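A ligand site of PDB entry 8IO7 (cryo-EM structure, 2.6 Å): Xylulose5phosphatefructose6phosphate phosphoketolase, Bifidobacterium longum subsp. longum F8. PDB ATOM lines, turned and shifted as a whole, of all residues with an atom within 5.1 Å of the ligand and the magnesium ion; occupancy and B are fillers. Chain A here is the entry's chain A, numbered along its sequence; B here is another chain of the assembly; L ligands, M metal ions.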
ATOM      1  N   GLY A  66      -2.105  24.444  34.882  1.00  0.00           N
ATOM      2  CA  GLY A  66      -1.596  23.309  35.637  1.00  0.00           C
ATOM      3  C   GLY A  66      -0.087  23.316  35.795  1.00  0.00           C
ATOM      4  O   GLY A  66       0.441  22.940  36.834  1.00  0.00           O
ATOM      5  N   THR A  67       0.623  23.761  34.765  1.00  0.00           N
ATOM      6  CA  THR A  67       2.079  23.765  34.783  1.00  0.00           C
ATOM      7  C   THR A  67       2.678  25.141  35.019  1.00  0.00           C
ATOM      8  O   THR A  67       3.885  25.243  35.216  1.00  0.00           O
ATOM      9  CB  THR A  67       2.622  23.206  33.462  1.00  0.00           C
ATOM     10  OG1 THR A  67       4.039  23.118  33.536  1.00  0.00           O
ATOM     11  CG2 THR A  67       2.242  24.120  32.315  1.00  0.00           C
ATOM     12  N   PRO A  95       6.924  21.825  28.345  1.00  0.00           N
ATOM     13  CA  PRO A  95       5.475  22.039  28.367  1.00  0.00           C
ATOM     14  C   PRO A  95       5.132  23.403  27.796  1.00  0.00           C
ATOM     15  O   PRO A  95       4.943  24.377  28.531  1.00  0.00           O
ATOM     16  CB  PRO A  95       5.128  21.943  29.862  1.00  0.00           C
ATOM     17  CG  PRO A  95       6.317  21.335  30.509  1.00  0.00           C
ATOM     18  CD  PRO A  95       7.483  21.762  29.704  1.00  0.00           C
ATOM     19  N   HIS A  97       2.518  24.552  26.634  1.00  0.00           N
ATOM     20  CA  HIS A  97       1.216  25.093  26.987  1.00  0.00           C
ATOM     21  C   HIS A  97       1.294  26.000  28.210  1.00  0.00           C
ATOM     22  O   HIS A  97       0.331  26.702  28.519  1.00  0.00           O
ATOM     23  CB  HIS A  97       0.219  23.967  27.215  1.00  0.00           C
ATOM     24  CG  HIS A  97       0.690  22.922  28.174  1.00  0.00           C
ATOM     25  ND1 HIS A  97       1.450  21.837  27.772  1.00  0.00           N
ATOM     26  CD2 HIS A  97       0.512  22.780  29.503  1.00  0.00           C
ATOM     27  CE1 HIS A  97       1.723  21.085  28.825  1.00  0.00           C
ATOM     28  NE2 HIS A  97       1.161  21.638  29.884  1.00  0.00           N
ATOM     29  N   GLY A 155       4.233  22.968  21.175  1.00  0.00           N
ATOM     30  CA  GLY A 155       2.947  22.462  20.778  1.00  0.00           C
ATOM     31  C   GLY A 155       2.977  20.981  20.786  1.00  0.00           C
ATOM     32  O   GLY A 155       2.248  20.366  21.445  1.00  0.00           O
ATOM     33  N   GLU A 156       3.869  20.428  20.070  1.00  0.00           N
ATOM     34  CA  GLU A 156       4.007  19.023  20.029  1.00  0.00           C
ATOM     35  C   GLU A 156       4.744  18.541  21.236  1.00  0.00           C
ATOM     36  O   GLU A 156       5.484  19.300  21.818  1.00  0.00           O
ATOM     37  CB  GLU A 156       4.863  18.743  18.848  1.00  0.00           C
ATOM     38  CG  GLU A 156       4.754  17.377  18.306  1.00  0.00           C
ATOM     39  CD  GLU A 156       3.418  16.916  18.601  1.00  0.00           C
ATOM     40  OE1 GLU A 156       2.526  17.657  18.218  1.00  0.00           O
ATOM     41  OE2 GLU A 156       3.277  15.917  19.302  1.00  0.00           O
ATOM     42  N   LEU A 157       4.654  17.271  21.603  1.00  0.00           N
ATOM     43  CA  LEU A 157       5.361  16.856  22.799  1.00  0.00           C
ATOM     44  C   LEU A 157       6.408  15.794  22.612  1.00  0.00           C
ATOM     45  O   LEU A 157       6.191  14.892  21.862  1.00  0.00           O
ATOM     46  CB  LEU A 157       4.379  16.485  23.860  1.00  0.00           C
ATOM     47  CG  LEU A 157       3.617  17.634  24.514  1.00  0.00           C
ATOM     48  CD1 LEU A 157       2.967  17.122  25.741  1.00  0.00           C
ATOM     49  CD2 LEU A 157       4.442  18.836  24.869  1.00  0.00           C
ATOM     50  N   GLY A 181       8.017  17.904  30.805  1.00  0.00           N
ATOM     51  CA  GLY A 181       6.822  17.457  31.483  1.00  0.00           C
ATOM     52  C   GLY A 181       6.836  15.956  31.711  1.00  0.00           C
ATOM     53  O   GLY A 181       7.311  15.172  30.880  1.00  0.00           O
ATOM     54  N   ASP A 182       6.317  15.539  32.859  1.00  0.00           N
ATOM     55  CA  ASP A 182       6.283  14.123  33.186  1.00  0.00           C
ATOM     56  C   ASP A 182       5.379  13.358  32.227  1.00  0.00           C
ATOM     57  O   ASP A 182       5.695  12.238  31.818  1.00  0.00           O
ATOM     58  CB  ASP A 182       5.833  13.922  34.624  1.00  0.00           C
ATOM     59  CG  ASP A 182       4.525  14.619  34.926  1.00  0.00           C
ATOM     60  OD1 ASP A 182       4.115  15.477  34.138  1.00  0.00           O
ATOM     61  OD2 ASP A 182       3.921  14.291  35.974  1.00  0.00           O
ATOM     62  N   GLY A 183       4.243  13.955  31.859  1.00  0.00           N
ATOM     63  CA  GLY A 183       3.418  13.363  30.817  1.00  0.00           C
ATOM     64  C   GLY A 183       4.117  13.363  29.475  1.00  0.00           C
ATOM     65  O   GLY A 183       4.022  12.398  28.713  1.00  0.00           O
ATOM     66  N   GLU A 184       4.835  14.441  29.171  1.00  0.00           N
ATOM     67  CA  GLU A 184       5.615  14.506  27.943  1.00  0.00           C
ATOM     68  C   GLU A 184       6.680  13.417  27.896  1.00  0.00           C
ATOM     69  O   GLU A 184       7.015  12.932  26.816  1.00  0.00           O
ATOM     70  CB  GLU A 184       6.231  15.892  27.802  1.00  0.00           C
ATOM     71  CG  GLU A 184       7.210  16.032  26.644  1.00  0.00           C
ATOM     72  CD  GLU A 184       7.765  17.437  26.544  1.00  0.00           C
ATOM     73  OE1 GLU A 184       8.599  17.695  25.650  1.00  0.00           O
ATOM     74  OE2 GLU A 184       7.371  18.281  27.377  1.00  0.00           O
ATOM     75  N   THR A 187       5.998  10.181  25.941  1.00  0.00           N
ATOM     76  CA  THR A 187       6.007  10.137  24.496  1.00  0.00           C
ATOM     77  C   THR A 187       7.220   9.376  23.987  1.00  0.00           C
ATOM     78  O   THR A 187       8.267   9.297  24.645  1.00  0.00           O
ATOM     79  CB  THR A 187       6.023  11.546  23.907  1.00  0.00           C
ATOM     80  OG1 THR A 187       7.191  12.220  24.352  1.00  0.00           O
ATOM     81  CG2 THR A 187       4.796  12.325  24.362  1.00  0.00           C
ATOM     82  N   HIS A 213       9.788  17.973  35.109  1.00  0.00           N
ATOM     83  CA  HIS A 213       8.706  18.624  35.837  1.00  0.00           C
ATOM     84  C   HIS A 213       7.670  17.571  36.197  1.00  0.00           C
ATOM     85  O   HIS A 213       6.618  17.440  35.568  1.00  0.00           O
ATOM     86  CB  HIS A 213       8.111  19.762  35.020  1.00  0.00           C
ATOM     87  CG  HIS A 213       7.110  20.584  35.764  1.00  0.00           C
ATOM     88  ND1 HIS A 213       6.245  21.440  35.130  1.00  0.00           N
ATOM     89  CD2 HIS A 213       6.851  20.680  37.086  1.00  0.00           C
ATOM     90  CE1 HIS A 213       5.482  22.031  36.034  1.00  0.00           C
ATOM     91  NE2 HIS A 213       5.827  21.586  37.231  1.00  0.00           N
ATOM     92  N   ASN A 215       5.039  16.793  37.928  1.00  0.00           N
ATOM     93  CA  ASN A 215       3.890  17.294  38.673  1.00  0.00           C
ATOM     94  C   ASN A 215       2.822  16.228  38.886  1.00  0.00           C
ATOM     95  O   ASN A 215       1.823  16.505  39.554  1.00  0.00           O
ATOM     96  CB  ASN A 215       3.274  18.503  37.961  1.00  0.00           C
ATOM     97  CG  ASN A 215       2.890  18.216  36.525  1.00  0.00           C
ATOM     98  OD1 ASN A 215       2.840  17.065  36.094  1.00  0.00           O
ATOM     99  ND2 ASN A 215       2.610  19.268  35.777  1.00  0.00           N
ATOM    100  N   GLY A 216       3.006  15.028  38.352  1.00  0.00           N
ATOM    101  CA  GLY A 216       2.163  13.899  38.665  1.00  0.00           C
ATOM    102  C   GLY A 216       1.126  13.488  37.642  1.00  0.00           C
ATOM    103  O   GLY A 216       0.848  12.298  37.507  1.00  0.00           O
ATOM    104  N   TYR A 217       0.541  14.445  36.925  1.00  0.00           N
ATOM    105  CA  TYR A 217      -0.612  14.160  36.103  1.00  0.00           C
ATOM    106  C   TYR A 217      -0.482  14.746  34.714  1.00  0.00           C
ATOM    107  O   TYR A 217       0.173  15.777  34.494  1.00  0.00           O
ATOM    108  CB  TYR A 217      -1.905  14.681  36.739  1.00  0.00           C
ATOM    109  CG  TYR A 217      -2.100  14.224  38.160  1.00  0.00           C
ATOM    110  CD1 TYR A 217      -1.547  14.928  39.212  1.00  0.00           C
ATOM    111  CD2 TYR A 217      -2.830  13.081  38.439  1.00  0.00           C
ATOM    112  CE1 TYR A 217      -1.709  14.504  40.500  1.00  0.00           C
ATOM    113  CE2 TYR A 217      -2.995  12.654  39.736  1.00  0.00           C
ATOM    114  CZ  TYR A 217      -2.442  13.378  40.762  1.00  0.00           C
ATOM    115  OH  TYR A 217      -2.607  12.960  42.061  1.00  0.00           O
ATOM    116  N   LYS A 218      -1.117  14.061  33.772  1.00  0.00           N
ATOM    117  CA  LYS A 218      -1.429  14.547  32.444  1.00  0.00           C
ATOM    118  C   LYS A 218      -2.794  15.222  32.499  1.00  0.00           C
ATOM    119  O   LYS A 218      -3.263  15.584  33.583  1.00  0.00           O
ATOM    120  CB  LYS A 218      -1.427  13.403  31.448  1.00  0.00           C
ATOM    121  CG  LYS A 218      -0.131  12.671  31.351  1.00  0.00           C
ATOM    122  CD  LYS A 218      -0.153  11.698  30.192  1.00  0.00           C
ATOM    123  CE  LYS A 218      -1.081  10.527  30.452  1.00  0.00           C
ATOM    124  NZ  LYS A 218      -0.514   9.590  31.456  1.00  0.00           N
ATOM    125  N   ILE A 219      -3.439  15.428  31.355  1.00  0.00           N
ATOM    126  CA  ILE A 219      -4.828  15.890  31.323  1.00  0.00           C
ATOM    127  C   ILE A 219      -5.705  14.711  31.729  1.00  0.00           C
ATOM    128  O   ILE A 219      -5.782  13.704  31.026  1.00  0.00           O
ATOM    129  CB  ILE A 219      -5.223  16.474  29.965  1.00  0.00           C
ATOM    130  CG1 ILE A 219      -5.135  15.445  28.836  1.00  0.00           C
ATOM    131  CG2 ILE A 219      -4.291  17.560  29.581  1.00  0.00           C
ATOM    132  CD1 ILE A 219      -5.741  15.931  27.542  1.00  0.00           C
ATOM    133  N   THR A 223       0.578  10.297  35.504  1.00  0.00           N
ATOM    134  CA  THR A 223       1.713   9.908  34.681  1.00  0.00           C
ATOM    135  C   THR A 223       2.372   8.657  35.228  1.00  0.00           C
ATOM    136  O   THR A 223       2.330   8.384  36.428  1.00  0.00           O
ATOM    137  CB  THR A 223       2.742  11.038  34.629  1.00  0.00           C
ATOM    138  OG1 THR A 223       3.314  11.229  35.921  1.00  0.00           O
ATOM    139  CG2 THR A 223       2.075  12.324  34.200  1.00  0.00           C
ATOM    140  N   LYS A 300       0.485  19.893  40.866  1.00  0.00           N
ATOM    141  CA  LYS A 300      -0.018  20.546  39.660  1.00  0.00           C
ATOM    142  C   LYS A 300      -0.906  21.719  40.036  1.00  0.00           C
ATOM    143  O   LYS A 300      -1.806  21.592  40.861  1.00  0.00           O
ATOM    144  CB  LYS A 300      -0.784  19.551  38.806  1.00  0.00           C
ATOM    145  CG  LYS A 300      -1.107  20.040  37.409  1.00  0.00           C
ATOM    146  CD  LYS A 300      -1.345  18.875  36.469  1.00  0.00           C
ATOM    147  CE  LYS A 300      -1.463  19.335  35.043  1.00  0.00           C
ATOM    148  NZ  LYS A 300      -1.311  18.215  34.083  1.00  0.00           N
ATOM    149  N   HIS A 320      -5.464  21.334  35.088  1.00  0.00           N
ATOM    150  CA  HIS A 320      -4.623  21.403  33.904  1.00  0.00           C
ATOM    151  C   HIS A 320      -4.918  22.649  33.081  1.00  0.00           C
ATOM    152  O   HIS A 320      -4.083  23.549  32.979  1.00  0.00           O
ATOM    153  CB  HIS A 320      -4.808  20.170  33.037  1.00  0.00           C
ATOM    154  CG  HIS A 320      -4.077  20.261  31.735  1.00  0.00           C
ATOM    155  ND1 HIS A 320      -2.723  19.997  31.621  1.00  0.00           N
ATOM    156  CD2 HIS A 320      -4.485  20.644  30.508  1.00  0.00           C
ATOM    157  CE1 HIS A 320      -2.343  20.178  30.373  1.00  0.00           C
ATOM    158  NE2 HIS A 320      -3.397  20.577  29.672  1.00  0.00           N
ATOM    159  N   PRO B 435      -4.587   8.388  23.375  1.00  0.00           N
ATOM    160  CA  PRO B 435      -3.400   9.044  23.964  1.00  0.00           C
ATOM    161  C   PRO B 435      -3.806  10.172  24.896  1.00  0.00           C
ATOM    162  O   PRO B 435      -3.658  11.360  24.578  1.00  0.00           O
ATOM    163  CB  PRO B 435      -2.647   9.525  22.728  1.00  0.00           C
ATOM    164  CG  PRO B 435      -3.695   9.717  21.698  1.00  0.00           C
ATOM    165  CD  PRO B 435      -4.718   8.651  21.937  1.00  0.00           C
ATOM    166  N   ASP B 436      -4.335   9.810  26.068  1.00  0.00           N
ATOM    167  CA  ASP B 436      -4.643  10.738  27.146  1.00  0.00           C
ATOM    168  C   ASP B 436      -5.803  11.666  26.800  1.00  0.00           C
ATOM    169  O   ASP B 436      -5.974  12.716  27.433  1.00  0.00           O
ATOM    170  CB  ASP B 436      -3.396  11.556  27.498  1.00  0.00           C
ATOM    171  CG  ASP B 436      -3.557  12.370  28.743  1.00  0.00           C
ATOM    172  OD1 ASP B 436      -4.407  12.016  29.578  1.00  0.00           O
ATOM    173  OD2 ASP B 436      -2.866  13.400  28.866  1.00  0.00           O
ATOM    174  N   GLU B 437      -6.635  11.317  25.822  1.00  0.00           N
ATOM    175  CA  GLU B 437      -7.575  12.264  25.236  1.00  0.00           C
ATOM    176  C   GLU B 437      -9.009  11.760  25.165  1.00  0.00           C
ATOM    177  O   GLU B 437      -9.832  12.375  24.490  1.00  0.00           O
ATOM    178  CB  GLU B 437      -7.072  12.658  23.845  1.00  0.00           C
ATOM    179  CG  GLU B 437      -5.782  13.449  23.894  1.00  0.00           C
ATOM    180  CD  GLU B 437      -5.269  13.812  22.529  1.00  0.00           C
ATOM    181  OE1 GLU B 437      -5.839  13.342  21.535  1.00  0.00           O
ATOM    182  OE2 GLU B 437      -4.283  14.580  22.458  1.00  0.00           O
ATOM    183  N   LEU B 477       0.314   8.837  27.146  1.00  0.00           N
ATOM    184  CA  LEU B 477       0.564   9.946  26.230  1.00  0.00           C
ATOM    185  C   LEU B 477       1.618   9.533  25.205  1.00  0.00           C
ATOM    186  O   LEU B 477       2.777   9.961  25.249  1.00  0.00           O
ATOM    187  CB  LEU B 477       0.969  11.194  26.999  1.00  0.00           C
ATOM    188  CG  LEU B 477       1.167  12.443  26.144  1.00  0.00           C
ATOM    189  CD1 LEU B 477      -0.042  12.641  25.271  1.00  0.00           C
ATOM    190  CD2 LEU B 477       1.380  13.634  27.040  1.00  0.00           C
ATOM    191  N   GLU B 479       1.075   8.352  20.969  1.00  0.00           N
ATOM    192  CA  GLU B 479       0.264   7.828  19.876  1.00  0.00           C
ATOM    193  C   GLU B 479       0.834   6.540  19.312  1.00  0.00           C
ATOM    194  O   GLU B 479       0.077   5.699  18.819  1.00  0.00           O
ATOM    195  CB  GLU B 479       0.132   8.888  18.771  1.00  0.00           C
ATOM    196  CG  GLU B 479      -0.714  10.078  19.156  1.00  0.00           C
ATOM    197  CD  GLU B 479       0.011  11.074  20.041  1.00  0.00           C
ATOM    198  OE1 GLU B 479       1.133  10.778  20.489  1.00  0.00           O
ATOM    199  OE2 GLU B 479      -0.562  12.156  20.306  1.00  0.00           O
ATOM    200  N   TYR B 501      -6.620  13.688  18.879  1.00  0.00           N
ATOM    201  CA  TYR B 501      -6.607  15.003  18.258  1.00  0.00           C
ATOM    202  C   TYR B 501      -6.206  14.866  16.793  1.00  0.00           C
ATOM    203  O   TYR B 501      -5.482  13.944  16.410  1.00  0.00           O
ATOM    204  CB  TYR B 501      -5.609  15.922  18.967  1.00  0.00           C
ATOM    205  CG  TYR B 501      -6.098  16.567  20.246  1.00  0.00           C
ATOM    206  CD1 TYR B 501      -7.095  15.979  21.011  1.00  0.00           C
ATOM    207  CD2 TYR B 501      -5.537  17.744  20.703  1.00  0.00           C
ATOM    208  CE1 TYR B 501      -7.528  16.564  22.179  1.00  0.00           C
ATOM    209  CE2 TYR B 501      -5.960  18.338  21.877  1.00  0.00           C
ATOM    210  CZ  TYR B 501      -6.958  17.741  22.606  1.00  0.00           C
ATOM    211  OH  TYR B 501      -7.381  18.325  23.777  1.00  0.00           O
ATOM    212  N   PHE B 504      -2.327  15.551  15.707  1.00  0.00           N
ATOM    213  CA  PHE B 504      -1.339  14.627  16.250  1.00  0.00           C
ATOM    214  C   PHE B 504      -1.372  13.256  15.588  1.00  0.00           C
ATOM    215  O   PHE B 504      -0.482  12.444  15.836  1.00  0.00           O
ATOM    216  CB  PHE B 504      -1.526  14.499  17.757  1.00  0.00           C
ATOM    217  CG  PHE B 504      -1.465  15.808  18.474  1.00  0.00           C
ATOM    218  CD1 PHE B 504      -0.702  16.848  17.962  1.00  0.00           C
ATOM    219  CD2 PHE B 504      -2.168  16.015  19.638  1.00  0.00           C
ATOM    220  CE1 PHE B 504      -0.653  18.057  18.600  1.00  0.00           C
ATOM    221  CE2 PHE B 504      -2.119  17.224  20.276  1.00  0.00           C
ATOM    222  CZ  PHE B 504      -1.347  18.243  19.761  1.00  0.00           C
ATOM    223  N   VAL B 507       1.678  11.981  13.922  1.00  0.00           N
ATOM    224  CA  VAL B 507       2.729  11.326  14.694  1.00  0.00           C
ATOM    225  C   VAL B 507       2.833   9.857  14.312  1.00  0.00           C
ATOM    226  O   VAL B 507       3.918   9.265  14.355  1.00  0.00           O
ATOM    227  CB  VAL B 507       2.461  11.519  16.199  1.00  0.00           C
ATOM    228  CG1 VAL B 507       3.429  10.708  17.037  1.00  0.00           C
ATOM    229  CG2 VAL B 507       2.562  12.987  16.562  1.00  0.00           C
ATOM    230  N   ASN B 549      -5.686  25.677  22.521  1.00  0.00           N
ATOM    231  CA  ASN B 549      -4.321  25.367  22.131  1.00  0.00           C
ATOM    232  C   ASN B 549      -3.788  26.358  21.096  1.00  0.00           C
ATOM    233  O   ASN B 549      -2.792  27.041  21.343  1.00  0.00           O
ATOM    234  CB  ASN B 549      -4.244  23.935  21.608  1.00  0.00           C
ATOM    235  CG  ASN B 549      -4.704  22.932  22.642  1.00  0.00           C
ATOM    236  OD1 ASN B 549      -4.291  22.983  23.801  1.00  0.00           O
ATOM    237  ND2 ASN B 549      -5.560  22.003  22.231  1.00  0.00           N
ATOM    238  N   HIS B 553      -1.796  23.246  17.214  1.00  0.00           N
ATOM    239  CA  HIS B 553      -2.659  22.073  17.252  1.00  0.00           C
ATOM    240  C   HIS B 553      -3.605  21.986  16.067  1.00  0.00           C
ATOM    241  O   HIS B 553      -4.497  21.133  16.066  1.00  0.00           O
ATOM    242  CB  HIS B 553      -3.469  22.081  18.548  1.00  0.00           C
ATOM    243  CG  HIS B 553      -2.648  21.781  19.765  1.00  0.00           C
ATOM    244  ND1 HIS B 553      -1.527  22.510  20.113  1.00  0.00           N
ATOM    245  CD2 HIS B 553      -2.809  20.857  20.749  1.00  0.00           C
ATOM    246  CE1 HIS B 553      -1.027  22.034  21.231  1.00  0.00           C
ATOM    247  NE2 HIS B 553      -1.785  21.030  21.635  1.00  0.00           N
HETATM  248  N1  LIG L   1      -0.283  14.292  22.378  1.00  0.00           N
HETATM  249  C1  LIG L   1       0.820  14.894  21.939  1.00  0.00           C
HETATM  250  C2  LIG L   1       1.830  14.041  21.255  1.00  0.00           C
HETATM  251  N2  LIG L   1       1.101  16.198  22.046  1.00  0.00           N
HETATM  252  C3  LIG L   1       0.197  16.978  22.654  1.00  0.00           C
HETATM  253  N3  LIG L   1       0.488  18.281  22.763  1.00  0.00           N
HETATM  254  C4  LIG L   1      -1.017  16.437  23.174  1.00  0.00           C
HETATM  255  C5  LIG L   1      -1.174  15.092  22.986  1.00  0.00           C
HETATM  256  C6  LIG L   1      -2.066  17.266  23.870  1.00  0.00           C
HETATM  257  N4  LIG L   1      -1.564  17.911  25.107  1.00  0.00           N
HETATM  258  C7  LIG L   1      -1.272  19.188  25.198  1.00  0.00           C
HETATM  259  S1  LIG L   1      -0.739  19.608  26.726  1.00  0.00           S
HETATM  260  C8  LIG L   1      -0.921  17.984  27.279  1.00  0.00           C
HETATM  261  C9  LIG L   1      -1.377  17.193  26.286  1.00  0.00           C
HETATM  262  C10 LIG L   1      -1.655  15.736  26.352  1.00  0.00           C
HETATM  263  C11 LIG L   1      -0.588  17.606  28.692  1.00  0.00           C
HETATM  264  C12 LIG L   1       0.893  17.695  28.988  1.00  0.00           C
HETATM  265  O1  LIG L   1       1.202  16.779  30.055  1.00  0.00           O
HETATM  266  P1  LIG L   1       2.433  16.930  31.015  1.00  0.00           P
HETATM  267  O2  LIG L   1       2.181  16.151  32.301  1.00  0.00           O
HETATM  268  O3  LIG L   1       3.674  16.618  30.296  1.00  0.00           O
HETATM  269  O4  LIG L   1       2.336  18.443  31.392  1.00  0.00           O
HETATM  270  P2  LIG L   1       1.931  19.356  32.619  1.00  0.00           P
HETATM  271  O5  LIG L   1       3.219  20.069  32.996  1.00  0.00           O
HETATM  272  O6  LIG L   1       1.358  18.532  33.728  1.00  0.00           O
HETATM  273  O7  LIG L   1       0.954  20.356  32.038  1.00  0.00           O
HETATM  274 MG    MG M   1       2.595  17.054  34.099  1.00  0.00          MG
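NE2 of His 97 is in hydrogen-bond range of O7 of the ligand (2.5 Å).
The backbone carbonyl oxygen (O) of Gly 155 lies within hydrogen-bond range of a nitrogen (N3) of the ligand (3.0 Å).
O3 of the ligand lies within hydrogen-bond range of N of Glu 184, at 2.7 Å.
O7 of the ligand is in salt-bridge range of NZ of Lys 300, at 3.7 Å.
O3 of the ligand is in hydrogen-bond range of N of Gly 183, 3.1 Å away.
The side-chain hydroxyl of Thr 67 is in hydrogen-bond range of an oxygen (O5) of the ligand, 3.2 Å away.
N of Asp 182 sits at hydrogen-bond distance from O of His 213 (3.3 Å).
The side-chain carboxylate (OD2) of Asp 182 lies within hydrogen-bond range of the side-chain hydroxyl (OG1) of Thr 223 (3.1 Å).
O of Lys 218 sits at hydrogen-bond distance from NZ of Lys 300 (3.3 Å).
The side-chain amide oxygen of Asn 215 sits close to the backbone carbonyl oxygen of Tyr 217, 3.4 Å away.
The side-chain carboxylate (OE1) of Glu 437 of chain B lies within hydrogen-bond range of the backbone NH (N) of Tyr 501 of chain B (2.8 Å).
O of Leu 477 of chain B sits close to N of Thr 187 (3.3 Å).
NZ of Lys 300 sits at hydrogen-bond distance from O of Tyr 217, 2.9 Å away.
The backbone carbonyl oxygen of His 320 is in hydrogen-bond range of the backbone NH of Gly 66.
The side-chain carboxylate (OE2) of Glu 479 of chain B lies close to a nitrogen (N1) of the ligand, 3.0 Å away.
Residues that only touch the ligand: Glu 156 (3.1 Å), Glu 437 of chain B (3.2 Å), Phe 504 of chain B (3.2 Å), Leu 477 of chain B (3.3 Å), Gly 181 (3.5 Å), His 320 (3.5 Å), Asp 436 of chain B (3.6 Å), Leu 157 (3.6 Å), His 553 of chain B (3.7 Å), Ile 219 (3.8 Å), His 213 (3.9 Å) and Lys 218 (3.95 Å).
Hydrophobic or aromatic side chains that line the ligand: His 97, Leu 157, Ile 219, His 320, Leu 477 of chain B and Phe 504 of chain B.
Of the 31 residues printed, 22 come within 4 Å of the ligand.
The nearest printed residue that does not touch the ligand is Pro 95 (4.1 Å).
Three residues have an atom within 4 Å of the magnesium ion: Asp 182, Asn 215 and Tyr 217.
The magnesium ion is bound by an oxygen (O6) of the ligand (2.0 Å), the side-chain amide oxygen of Asn 215 (2.0 Å), an oxygen (O2) of the ligand (2.1 Å) and the side-chain carboxylate of Asp 182 (2.2 Å).
The magnesium ion has four donor atoms within binding distance.
Slightly farther from the magnesium ion lies the backbone carbonyl oxygen (O) of Tyr 217 (2.8 Å).
Slightly farther from the magnesium ion lies the side-chain amide nitrogen (ND2) of Asn 215 (2.8 Å).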
